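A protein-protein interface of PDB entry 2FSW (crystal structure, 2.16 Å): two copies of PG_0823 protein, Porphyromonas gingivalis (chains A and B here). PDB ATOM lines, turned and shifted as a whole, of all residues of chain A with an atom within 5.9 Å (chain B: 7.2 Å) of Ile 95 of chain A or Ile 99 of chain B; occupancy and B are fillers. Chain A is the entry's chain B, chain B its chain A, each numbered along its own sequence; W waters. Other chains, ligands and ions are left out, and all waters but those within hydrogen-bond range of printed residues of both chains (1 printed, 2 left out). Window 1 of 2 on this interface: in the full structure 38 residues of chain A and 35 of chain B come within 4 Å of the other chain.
Water W1 lies within hydrogen-bond range of NZ of Lys 91 of chain A and OE1 of Glu 105 of chain B.
Printed residues of chain B within 4 Å of Met 19 of chain A: Leu 28 (3.9 Å). Printed residues of chain B within 4 Å of Pro 94 of chain A: Glu 98 (3.5 Å). Of the printed residues of chain B, Ile 95 of chain A touches Glu 98, Ile 99 and Phe 102. Printed residues of chain B within 4 Å of Glu 98 of chain A: Pro 94, Ile 95 and Glu 98. Leu 93 of chain B touches none of the printed residues of chain A. Of chain A, only Ser 18 and Ile 95 come within 4 Å of Ile 99 of chain B. Of the printed residues of chain A, Phe 102 of chain B touches Ser 18, Phe 22, Lys 91, Val 92 and Ile 95. Printed residues of chain A within 4 Å of Met 104 of chain B: Pro 14. The nearest residue of chain A that does not touch Ile 99 of chain B is Pro 14 of chain A (4.1 Å).
Hydrophobic or aromatic side chains of chain A that line the printed part of chain B: Pro 14, Val 15, Met 19, Phe 22, Val 92, Pro 94, Ile 95 and Ile 99. Among the printed residues, 20 pairs touch across the chains. Among the printed residues, no Asp or Glu carboxylate lies within 4 Å of a Lys or Arg side-chain nitrogen of the other chain.
O of Ile 99 of chain B lies within hydrogen-bond range of OG of Ser 18 of chain A. OG of Ser 18 of chain A lies close to N of Gly 103 of chain B, at 3.3 Å.
The backbone carbonyl oxygen (O) of Pro 14 of chain A is in hydrogen-bond range of the side-chain hydroxyl (OG) of Ser 18 of chain A, at 3.0 Å.
Among the printed residues, pairs that only touch across the chains: Pro 14 of chain A with Gly 103 of chain B (3.4 Å), Pro 94 of chain A with Glu 98 of chain B (3.5 Å), Pro 14 of chain A with Ala 100 of chain B (3.6 Å), Glu 98 of chain A with Pro 94 of chain B (3.6 Å), Ile 99 of chain A with Ile 95 of chain B (3.6 Å), Val 15 of chain A with Ala 100 of chain B (3.6 Å), Val 92 of chain A with Phe 102 of chain B (3.7 Å), Ile 95 of chain A with Ile 99 of chain B (3.7 Å), Glu 98 of chain A with Ile 95 of chain B (3.7 Å), Pro 14 of chain A with Met 104 of chain B (3.7 Å), Ser 18 of chain A with Phe 102 of chain B (3.7 Å), Ile 95 of chain A with Glu 98 of chain B (3.7 Å), Glu 98 of chain A with Glu 98 of chain B (3.7 Å), Phe 22 of chain A with Phe 102 of chain B (3.8 Å), Lys 91 of chain A with Phe 102 of chain B (3.8 Å), Ser 18 of chain A with Leu 107 of chain B (3.8 Å), Met 19 of chain A with Leu 28 of chain B (3.9 Å) and Ile 95 of chain A with Phe 102 of chain B (3.96 Å).
Pro 94 of chain A touches Glu 98 of chain B, and with the chains exchanged Glu 98 of chain A touches Pro 94 of chain B. Ile 95 of chain A touches Glu 98 of chain B, and with the chains exchanged Glu 98 of chain A touches Ile 95 of chain B. Ile 95 of chain A touches Ile 99 of chain B, and with the chains exchanged Ile 99 of chain A touches Ile 95 of chain B. Glu 98 of chain A touches its own counterpart, Glu 98 of chain B. Positions printed for both chains: 28, 92, 93, 94, 95, 96, 97, 98, 99 and 100. Of the 20 pairs that touch across the chains among the printed residues, 7 have their exchanged pair printed and touching as well.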
ATOM      1  N   PRO A  14       3.458  16.531   4.773  1.00  0.00           N
ATOM      2  CA  PRO A  14       2.354  16.008   5.585  1.00  0.00           C
ATOM      3  C   PRO A  14       2.676  16.069   7.086  1.00  0.00           C
ATOM      4  O   PRO A  14       1.774  16.239   7.908  1.00  0.00           O
ATOM      5  CB  PRO A  14       2.206  14.557   5.091  1.00  0.00           C
ATOM      6  CG  PRO A  14       3.522  14.216   4.471  1.00  0.00           C
ATOM      7  CD  PRO A  14       4.038  15.498   3.889  1.00  0.00           C
ATOM      8  N   VAL A  15       3.960  15.978   7.424  1.00  0.00           N
ATOM      9  CA  VAL A  15       4.403  16.053   8.813  1.00  0.00           C
ATOM     10  C   VAL A  15       4.361  17.507   9.297  1.00  0.00           C
ATOM     11  O   VAL A  15       3.859  17.792  10.385  1.00  0.00           O
ATOM     12  CB  VAL A  15       5.819  15.416   8.992  1.00  0.00           C
ATOM     13  CG1 VAL A  15       6.316  15.552  10.432  1.00  0.00           C
ATOM     14  CG2 VAL A  15       5.784  13.965   8.577  1.00  0.00           C
ATOM     15  N   SER A  18       0.850  18.640   9.799  1.00  0.00           N
ATOM     16  CA  SER A  18       0.295  18.081  11.045  1.00  0.00           C
ATOM     17  C   SER A  18       0.761  18.824  12.282  1.00  0.00           C
ATOM     18  O   SER A  18      -0.032  19.065  13.197  1.00  0.00           O
ATOM     19  CB  SER A  18       0.603  16.601  11.157  1.00  0.00           C
ATOM     20  OG  SER A  18      -0.173  15.888  10.226  1.00  0.00           O
ATOM     21  N   MET A  19       2.048  19.190  12.291  1.00  0.00           N
ATOM     22  CA  MET A  19       2.642  19.929  13.404  1.00  0.00           C
ATOM     23  C   MET A  19       2.052  21.332  13.622  1.00  0.00           C
ATOM     24  O   MET A  19       2.146  21.868  14.726  1.00  0.00           O
ATOM     25  CB  MET A  19       4.172  19.971  13.301  1.00  0.00           C
ATOM     26  CG  MET A  19       4.867  18.608  13.459  1.00  0.00           C
ATOM     27  SD  MET A  19       4.056  17.351  14.747  1.00  0.00           S
ATOM     28  CE  MET A  19       4.037  18.417  16.362  1.00  0.00           C
ATOM     29  N   PHE A  22      -0.630  20.072  16.027  1.00  0.00           N
ATOM     30  CA  PHE A  22      -0.202  19.251  17.169  1.00  0.00           C
ATOM     31  C   PHE A  22       0.960  19.815  17.971  1.00  0.00           C
ATOM     32  O   PHE A  22       1.311  19.250  19.011  1.00  0.00           O
ATOM     33  CB  PHE A  22       0.211  17.834  16.716  1.00  0.00           C
ATOM     34  CG  PHE A  22      -0.868  17.057  16.020  1.00  0.00           C
ATOM     35  CD1 PHE A  22      -0.544  16.217  14.947  1.00  0.00           C
ATOM     36  CD2 PHE A  22      -2.198  17.120  16.444  1.00  0.00           C
ATOM     37  CE1 PHE A  22      -1.529  15.486  14.287  1.00  0.00           C
ATOM     38  CE2 PHE A  22      -3.202  16.387  15.773  1.00  0.00           C
ATOM     39  CZ  PHE A  22      -2.854  15.568  14.693  1.00  0.00           C
ATOM     40  N   LEU A  28      -1.998  17.436  22.183  1.00  0.00           N
ATOM     41  CA  LEU A  28      -2.081  15.981  22.134  1.00  0.00           C
ATOM     42  C   LEU A  28      -2.486  15.362  23.463  1.00  0.00           C
ATOM     43  O   LEU A  28      -3.143  14.317  23.482  1.00  0.00           O
ATOM     44  CB  LEU A  28      -0.757  15.378  21.637  1.00  0.00           C
ATOM     45  CG  LEU A  28      -0.503  15.644  20.156  1.00  0.00           C
ATOM     46  CD1 LEU A  28       0.934  15.293  19.765  1.00  0.00           C
ATOM     47  CD2 LEU A  28      -1.536  14.870  19.313  1.00  0.00           C
ATOM     48  N   LYS A  91      -8.825   9.928  14.736  1.00  0.00           N
ATOM     49  CA  LYS A  91      -7.671   9.559  13.892  1.00  0.00           C
ATOM     50  C   LYS A  91      -6.312   9.992  14.459  1.00  0.00           C
ATOM     51  O   LYS A  91      -5.252   9.602  13.925  1.00  0.00           O
ATOM     52  CB  LYS A  91      -7.796  10.116  12.465  1.00  0.00           C
ATOM     53  CG  LYS A  91      -9.079   9.754  11.736  1.00  0.00           C
ATOM     54  CD  LYS A  91      -9.022   8.339  11.241  1.00  0.00           C
ATOM     55  CE  LYS A  91     -10.169   8.055  10.310  1.00  0.00           C
ATOM     56  NZ  LYS A  91      -9.935   8.737   9.009  1.00  0.00           N
ATOM     57  N   VAL A  92      -6.347  10.823  15.495  1.00  0.00           N
ATOM     58  CA  VAL A  92      -5.124  11.237  16.223  1.00  0.00           C
ATOM     59  C   VAL A  92      -4.679  10.197  17.263  1.00  0.00           C
ATOM     60  O   VAL A  92      -3.503  10.113  17.590  1.00  0.00           O
ATOM     61  CB  VAL A  92      -5.331  12.622  16.908  1.00  0.00           C
ATOM     62  CG1 VAL A  92      -4.056  13.116  17.575  1.00  0.00           C
ATOM     63  CG2 VAL A  92      -5.823  13.620  15.896  1.00  0.00           C
ATOM     64  N   LEU A  93      -5.610   9.386  17.762  1.00  0.00           N
ATOM     65  CA  LEU A  93      -5.274   8.369  18.776  1.00  0.00           C
ATOM     66  C   LEU A  93      -4.145   7.393  18.414  1.00  0.00           C
ATOM     67  O   LEU A  93      -3.364   7.048  19.289  1.00  0.00           O
ATOM     68  CB  LEU A  93      -6.533   7.628  19.276  1.00  0.00           C
ATOM     69  CG  LEU A  93      -7.542   8.535  20.021  1.00  0.00           C
ATOM     70  CD1 LEU A  93      -8.854   7.773  20.302  1.00  0.00           C
ATOM     71  CD2 LEU A  93      -6.992   9.165  21.315  1.00  0.00           C
ATOM     72  N   PRO A  94      -4.046   6.930  17.143  1.00  0.00           N
ATOM     73  CA  PRO A  94      -2.859   6.130  16.777  1.00  0.00           C
ATOM     74  C   PRO A  94      -1.502   6.830  16.958  1.00  0.00           C
ATOM     75  O   PRO A  94      -0.502   6.163  17.250  1.00  0.00           O
ATOM     76  CB  PRO A  94      -3.106   5.798  15.290  1.00  0.00           C
ATOM     77  CG  PRO A  94      -4.564   5.888  15.133  1.00  0.00           C
ATOM     78  CD  PRO A  94      -4.978   7.032  16.007  1.00  0.00           C
ATOM     79  N   ILE A  95      -1.456   8.145  16.778  1.00  0.00           N
ATOM     80  CA  ILE A  95      -0.231   8.913  17.029  1.00  0.00           C
ATOM     81  C   ILE A  95       0.098   8.852  18.520  1.00  0.00           C
ATOM     82  O   ILE A  95       1.244   8.653  18.904  1.00  0.00           O
ATOM     83  CB  ILE A  95      -0.371  10.428  16.611  1.00  0.00           C
ATOM     84  CG1 ILE A  95      -0.661  10.565  15.101  1.00  0.00           C
ATOM     85  CG2 ILE A  95       0.906  11.255  17.048  1.00  0.00           C
ATOM     86  CD1 ILE A  95      -1.375  11.855  14.726  1.00  0.00           C
ATOM     87  N   ILE A  96      -0.938   9.025  19.335  1.00  0.00           N
ATOM     88  CA  ILE A  96      -0.830   9.076  20.771  1.00  0.00           C
ATOM     89  C   ILE A  96      -0.447   7.722  21.384  1.00  0.00           C
ATOM     90  O   ILE A  96       0.363   7.679  22.313  1.00  0.00           O
ATOM     91  CB  ILE A  96      -2.119   9.671  21.366  1.00  0.00           C
ATOM     92  CG1 ILE A  96      -2.177  11.176  21.006  1.00  0.00           C
ATOM     93  CG2 ILE A  96      -2.177   9.457  22.900  1.00  0.00           C
ATOM     94  CD1 ILE A  96      -3.562  11.841  21.327  1.00  0.00           C
ATOM     95  N   ASP A  97      -1.014   6.634  20.869  1.00  0.00           N
ATOM     96  CA  ASP A  97      -0.574   5.280  21.218  1.00  0.00           C
ATOM     97  C   ASP A  97       0.935   5.126  21.059  1.00  0.00           C
ATOM     98  O   ASP A  97       1.617   4.575  21.940  1.00  0.00           O
ATOM     99  CB  ASP A  97      -1.235   4.237  20.303  1.00  0.00           C
ATOM    100  CG  ASP A  97      -2.700   4.018  20.617  1.00  0.00           C
ATOM    101  OD1 ASP A  97      -3.155   4.412  21.704  1.00  0.00           O
ATOM    102  OD2 ASP A  97      -3.388   3.398  19.775  1.00  0.00           O
ATOM    103  N   GLU A  98       1.454   5.607  19.929  1.00  0.00           N
ATOM    104  CA  GLU A  98       2.878   5.533  19.696  1.00  0.00           C
ATOM    105  C   GLU A  98       3.701   6.423  20.659  1.00  0.00           C
ATOM    106  O   GLU A  98       4.817   6.050  21.034  1.00  0.00           O
ATOM    107  CB  GLU A  98       3.232   5.828  18.222  1.00  0.00           C
ATOM    108  CG  GLU A  98       2.848   4.756  17.203  1.00  0.00           C
ATOM    109  CD  GLU A  98       3.374   3.336  17.509  1.00  0.00           C
ATOM    110  OE1 GLU A  98       4.527   3.123  17.961  1.00  0.00           O
ATOM    111  OE2 GLU A  98       2.604   2.390  17.262  1.00  0.00           O
ATOM    112  N   ILE A  99       3.170   7.600  21.006  1.00  0.00           N
ATOM    113  CA  ILE A  99       3.818   8.486  21.970  1.00  0.00           C
ATOM    114  C   ILE A  99       3.850   7.866  23.364  1.00  0.00           C
ATOM    115  O   ILE A  99       4.885   7.929  24.062  1.00  0.00           O
ATOM    116  CB  ILE A  99       3.166   9.911  21.977  1.00  0.00           C
ATOM    117  CG1 ILE A  99       3.386  10.603  20.620  1.00  0.00           C
ATOM    118  CG2 ILE A  99       3.747  10.780  23.094  1.00  0.00           C
ATOM    119  CD1 ILE A  99       2.522  11.883  20.391  1.00  0.00           C
ATOM    120  N   ALA A 100       2.738   7.240  23.755  1.00  0.00           N
ATOM    121  CA  ALA A 100       2.654   6.541  25.037  1.00  0.00           C
ATOM    122  C   ALA A 100       3.677   5.413  25.105  1.00  0.00           C
ATOM    123  O   ALA A 100       4.392   5.260  26.114  1.00  0.00           O
ATOM    124  CB  ALA A 100       1.240   5.983  25.255  1.00  0.00           C
ATOM    125  N   LEU B  28      10.015  17.388  16.116  1.00  0.00           N
ATOM    126  CA  LEU B  28       9.664  16.210  15.336  1.00  0.00           C
ATOM    127  C   LEU B  28      10.005  16.353  13.859  1.00  0.00           C
ATOM    128  O   LEU B  28      10.371  15.388  13.215  1.00  0.00           O
ATOM    129  CB  LEU B  28       8.180  15.857  15.536  1.00  0.00           C
ATOM    130  CG  LEU B  28       7.775  15.399  16.966  1.00  0.00           C
ATOM    131  CD1 LEU B  28       6.244  15.216  17.106  1.00  0.00           C
ATOM    132  CD2 LEU B  28       8.495  14.119  17.304  1.00  0.00           C
ATOM    133  N   VAL B  92      11.646   7.348  17.804  1.00  0.00           N
ATOM    134  CA  VAL B  92      10.658   8.397  17.569  1.00  0.00           C
ATOM    135  C   VAL B  92      10.007   8.274  16.178  1.00  0.00           C
ATOM    136  O   VAL B  92       8.937   8.816  15.953  1.00  0.00           O
ATOM    137  CB  VAL B  92      11.282   9.820  17.765  1.00  0.00           C
ATOM    138  CG1 VAL B  92      10.248  10.949  17.562  1.00  0.00           C
ATOM    139  CG2 VAL B  92      11.979   9.937  19.157  1.00  0.00           C
ATOM    140  N   LEU B  93      10.657   7.562  15.256  1.00  0.00           N
ATOM    141  CA  LEU B  93      10.152   7.420  13.879  1.00  0.00           C
ATOM    142  C   LEU B  93       8.769   6.777  13.739  1.00  0.00           C
ATOM    143  O   LEU B  93       8.029   7.185  12.882  1.00  0.00           O
ATOM    144  CB  LEU B  93      11.190   6.724  12.953  1.00  0.00           C
ATOM    145  CG  LEU B  93      12.435   7.615  12.722  1.00  0.00           C
ATOM    146  CD1 LEU B  93      13.621   6.893  12.011  1.00  0.00           C
ATOM    147  CD2 LEU B  93      12.044   8.884  11.965  1.00  0.00           C
ATOM    148  N   PRO B  94       8.422   5.748  14.557  1.00  0.00           N
ATOM    149  CA  PRO B  94       7.031   5.256  14.515  1.00  0.00           C
ATOM    150  C   PRO B  94       5.963   6.314  14.873  1.00  0.00           C
ATOM    151  O   PRO B  94       4.857   6.260  14.327  1.00  0.00           O
ATOM    152  CB  PRO B  94       7.020   4.103  15.542  1.00  0.00           C
ATOM    153  CG  PRO B  94       8.421   3.710  15.680  1.00  0.00           C
ATOM    154  CD  PRO B  94       9.259   4.937  15.462  1.00  0.00           C
ATOM    155  N   ILE B  95       6.274   7.230  15.795  1.00  0.00           N
ATOM    156  CA  ILE B  95       5.383   8.363  16.082  1.00  0.00           C
ATOM    157  C   ILE B  95       5.159   9.195  14.820  1.00  0.00           C
ATOM    158  O   ILE B  95       4.026   9.458  14.425  1.00  0.00           O
ATOM    159  CB  ILE B  95       5.935   9.286  17.224  1.00  0.00           C
ATOM    160  CG1 ILE B  95       6.027   8.503  18.543  1.00  0.00           C
ATOM    161  CG2 ILE B  95       5.049  10.506  17.407  1.00  0.00           C
ATOM    162  CD1 ILE B  95       7.019   9.088  19.549  1.00  0.00           C
ATOM    163  N   ILE B  96       6.272   9.568  14.204  1.00  0.00           N
ATOM    164  CA  ILE B  96       6.301  10.409  13.046  1.00  0.00           C
ATOM    165  C   ILE B  96       5.617   9.754  11.829  1.00  0.00           C
ATOM    166  O   ILE B  96       4.944  10.449  11.060  1.00  0.00           O
ATOM    167  CB  ILE B  96       7.771  10.830  12.726  1.00  0.00           C
ATOM    168  CG1 ILE B  96       8.326  11.699  13.859  1.00  0.00           C
ATOM    169  CG2 ILE B  96       7.853  11.546  11.388  1.00  0.00           C
ATOM    170  CD1 ILE B  96       9.872  11.917  13.812  1.00  0.00           C
ATOM    171  N   ASP B  97       5.790   8.441  11.642  1.00  0.00           N
ATOM    172  CA  ASP B  97       5.021   7.716  10.624  1.00  0.00           C
ATOM    173  C   ASP B  97       3.500   7.906  10.812  1.00  0.00           C
ATOM    174  O   ASP B  97       2.765   8.040   9.845  1.00  0.00           O
ATOM    175  CB  ASP B  97       5.305   6.224  10.668  1.00  0.00           C
ATOM    176  CG  ASP B  97       6.670   5.852  10.108  1.00  0.00           C
ATOM    177  OD1 ASP B  97       7.359   6.709   9.484  1.00  0.00           O
ATOM    178  OD2 ASP B  97       7.051   4.677  10.315  1.00  0.00           O
ATOM    179  N   GLU B  98       3.022   7.857  12.048  1.00  0.00           N
ATOM    180  CA  GLU B  98       1.591   8.043  12.279  1.00  0.00           C
ATOM    181  C   GLU B  98       1.150   9.488  11.986  1.00  0.00           C
ATOM    182  O   GLU B  98       0.021   9.713  11.513  1.00  0.00           O
ATOM    183  CB  GLU B  98       1.162   7.641  13.707  1.00  0.00           C
ATOM    184  CG  GLU B  98       1.386   6.205  14.105  1.00  0.00           C
ATOM    185  CD  GLU B  98       0.343   5.211  13.571  1.00  0.00           C
ATOM    186  OE1 GLU B  98      -0.587   5.579  12.810  1.00  0.00           O
ATOM    187  OE2 GLU B  98       0.454   4.029  13.947  1.00  0.00           O
ATOM    188  N   ILE B  99       2.019  10.452  12.292  1.00  0.00           N
ATOM    189  CA  ILE B  99       1.765  11.871  11.983  1.00  0.00           C
ATOM    190  C   ILE B  99       1.734  12.127  10.476  1.00  0.00           C
ATOM    191  O   ILE B  99       0.894  12.875  10.006  1.00  0.00           O
ATOM    192  CB  ILE B  99       2.797  12.802  12.654  1.00  0.00           C
ATOM    193  CG1 ILE B  99       2.602  12.829  14.181  1.00  0.00           C
ATOM    194  CG2 ILE B  99       2.725  14.229  12.115  1.00  0.00           C
ATOM    195  CD1 ILE B  99       3.861  13.258  14.916  1.00  0.00           C
ATOM    196  N   ALA B 100       2.659  11.509   9.739  1.00  0.00           N
ATOM    197  CA  ALA B 100       2.720  11.651   8.279  1.00  0.00           C
ATOM    198  C   ALA B 100       1.444  11.087   7.683  1.00  0.00           C
ATOM    199  O   ALA B 100       0.843  11.699   6.805  1.00  0.00           O
ATOM    200  CB  ALA B 100       3.984  10.941   7.683  1.00  0.00           C
ATOM    201  N   LYS B 101       1.025   9.929   8.200  1.00  0.00           N
ATOM    202  CA  LYS B 101      -0.228   9.287   7.806  1.00  0.00           C
ATOM    203  C   LYS B 101      -1.449  10.209   8.044  1.00  0.00           C
ATOM    204  O   LYS B 101      -2.300  10.375   7.165  1.00  0.00           O
ATOM    205  CB  LYS B 101      -0.380   7.962   8.576  1.00  0.00           C
ATOM    206  CG  LYS B 101      -1.617   7.196   8.186  1.00  0.00           C
ATOM    207  CD  LYS B 101      -1.857   5.974   9.015  1.00  0.00           C
ATOM    208  CE  LYS B 101      -3.111   5.289   8.456  1.00  0.00           C
ATOM    209  NZ  LYS B 101      -3.864   4.574   9.507  1.00  0.00           N
ATOM    210  N   PHE B 102      -1.533  10.804   9.232  1.00  0.00           N
ATOM    211  CA  PHE B 102      -2.595  11.771   9.515  1.00  0.00           C
ATOM    212  C   PHE B 102      -2.556  12.949   8.525  1.00  0.00           C
ATOM    213  O   PHE B 102      -3.593  13.373   8.033  1.00  0.00           O
ATOM    214  CB  PHE B 102      -2.554  12.267  10.973  1.00  0.00           C
ATOM    215  CG  PHE B 102      -3.675  13.235  11.322  1.00  0.00           C
ATOM    216  CD1 PHE B 102      -4.851  12.777  11.926  1.00  0.00           C
ATOM    217  CD2 PHE B 102      -3.560  14.602  11.041  1.00  0.00           C
ATOM    218  CE1 PHE B 102      -5.884  13.650  12.246  1.00  0.00           C
ATOM    219  CE2 PHE B 102      -4.605  15.495  11.356  1.00  0.00           C
ATOM    220  CZ  PHE B 102      -5.760  15.016  11.959  1.00  0.00           C
ATOM    221  N   GLY B 103      -1.358  13.466   8.246  1.00  0.00           N
ATOM    222  CA  GLY B 103      -1.203  14.618   7.368  1.00  0.00           C
ATOM    223  C   GLY B 103      -1.672  14.319   5.960  1.00  0.00           C
ATOM    224  O   GLY B 103      -2.435  15.104   5.380  1.00  0.00           O
ATOM    225  N   MET B 104      -1.238  13.209   5.372  1.00  0.00           N
ATOM    226  CA  MET B 104      -1.647  12.959   3.990  1.00  0.00           C
ATOM    227  C   MET B 104      -3.100  12.494   3.820  1.00  0.00           C
ATOM    228  O   MET B 104      -3.668  12.653   2.745  1.00  0.00           O
ATOM    229  CB  MET B 104      -0.640  12.095   3.199  1.00  0.00           C
ATOM    230  CG  MET B 104      -0.172  10.809   3.834  1.00  0.00           C
ATOM    231  SD  MET B 104       1.239   9.944   2.739  1.00  0.00           S
ATOM    232  CE  MET B 104       2.786  10.638   3.600  1.00  0.00           C
ATOM    233  N   GLU B 105      -3.708  11.954   4.874  1.00  0.00           N
ATOM    234  CA  GLU B 105      -5.073  11.460   4.752  1.00  0.00           C
ATOM    235  C   GLU B 105      -6.130  12.527   4.999  1.00  0.00           C
ATOM    236  O   GLU B 105      -7.177  12.503   4.366  1.00  0.00           O
ATOM    237  CB  GLU B 105      -5.340  10.267   5.666  1.00  0.00           C
ATOM    238  CG  GLU B 105      -4.778   8.944   5.144  1.00  0.00           C
ATOM    239  CD  GLU B 105      -5.008   7.775   6.096  1.00  0.00           C
ATOM    240  OE1 GLU B 105      -5.709   7.923   7.126  1.00  0.00           O
ATOM    241  OE2 GLU B 105      -4.486   6.688   5.802  1.00  0.00           O
ATOM    242  N   LEU B 107      -5.283  16.108   5.726  1.00  0.00           N
ATOM    243  CA  LEU B 107      -4.890  17.489   5.529  1.00  0.00           C
ATOM    244  C   LEU B 107      -4.526  17.739   4.061  1.00  0.00           C
ATOM    245  O   LEU B 107      -3.877  18.725   3.734  1.00  0.00           O
ATOM    246  CB  LEU B 107      -3.759  17.883   6.496  1.00  0.00           C
ATOM    247  CG  LEU B 107      -3.986  17.758   8.019  1.00  0.00           C
ATOM    248  CD1 LEU B 107      -2.787  18.260   8.776  1.00  0.00           C
ATOM    249  CD2 LEU B 107      -5.241  18.522   8.479  1.00  0.00           C
HETATM  250  O   HOH W   1      -8.260   8.495   7.122  1.00  0.00           O
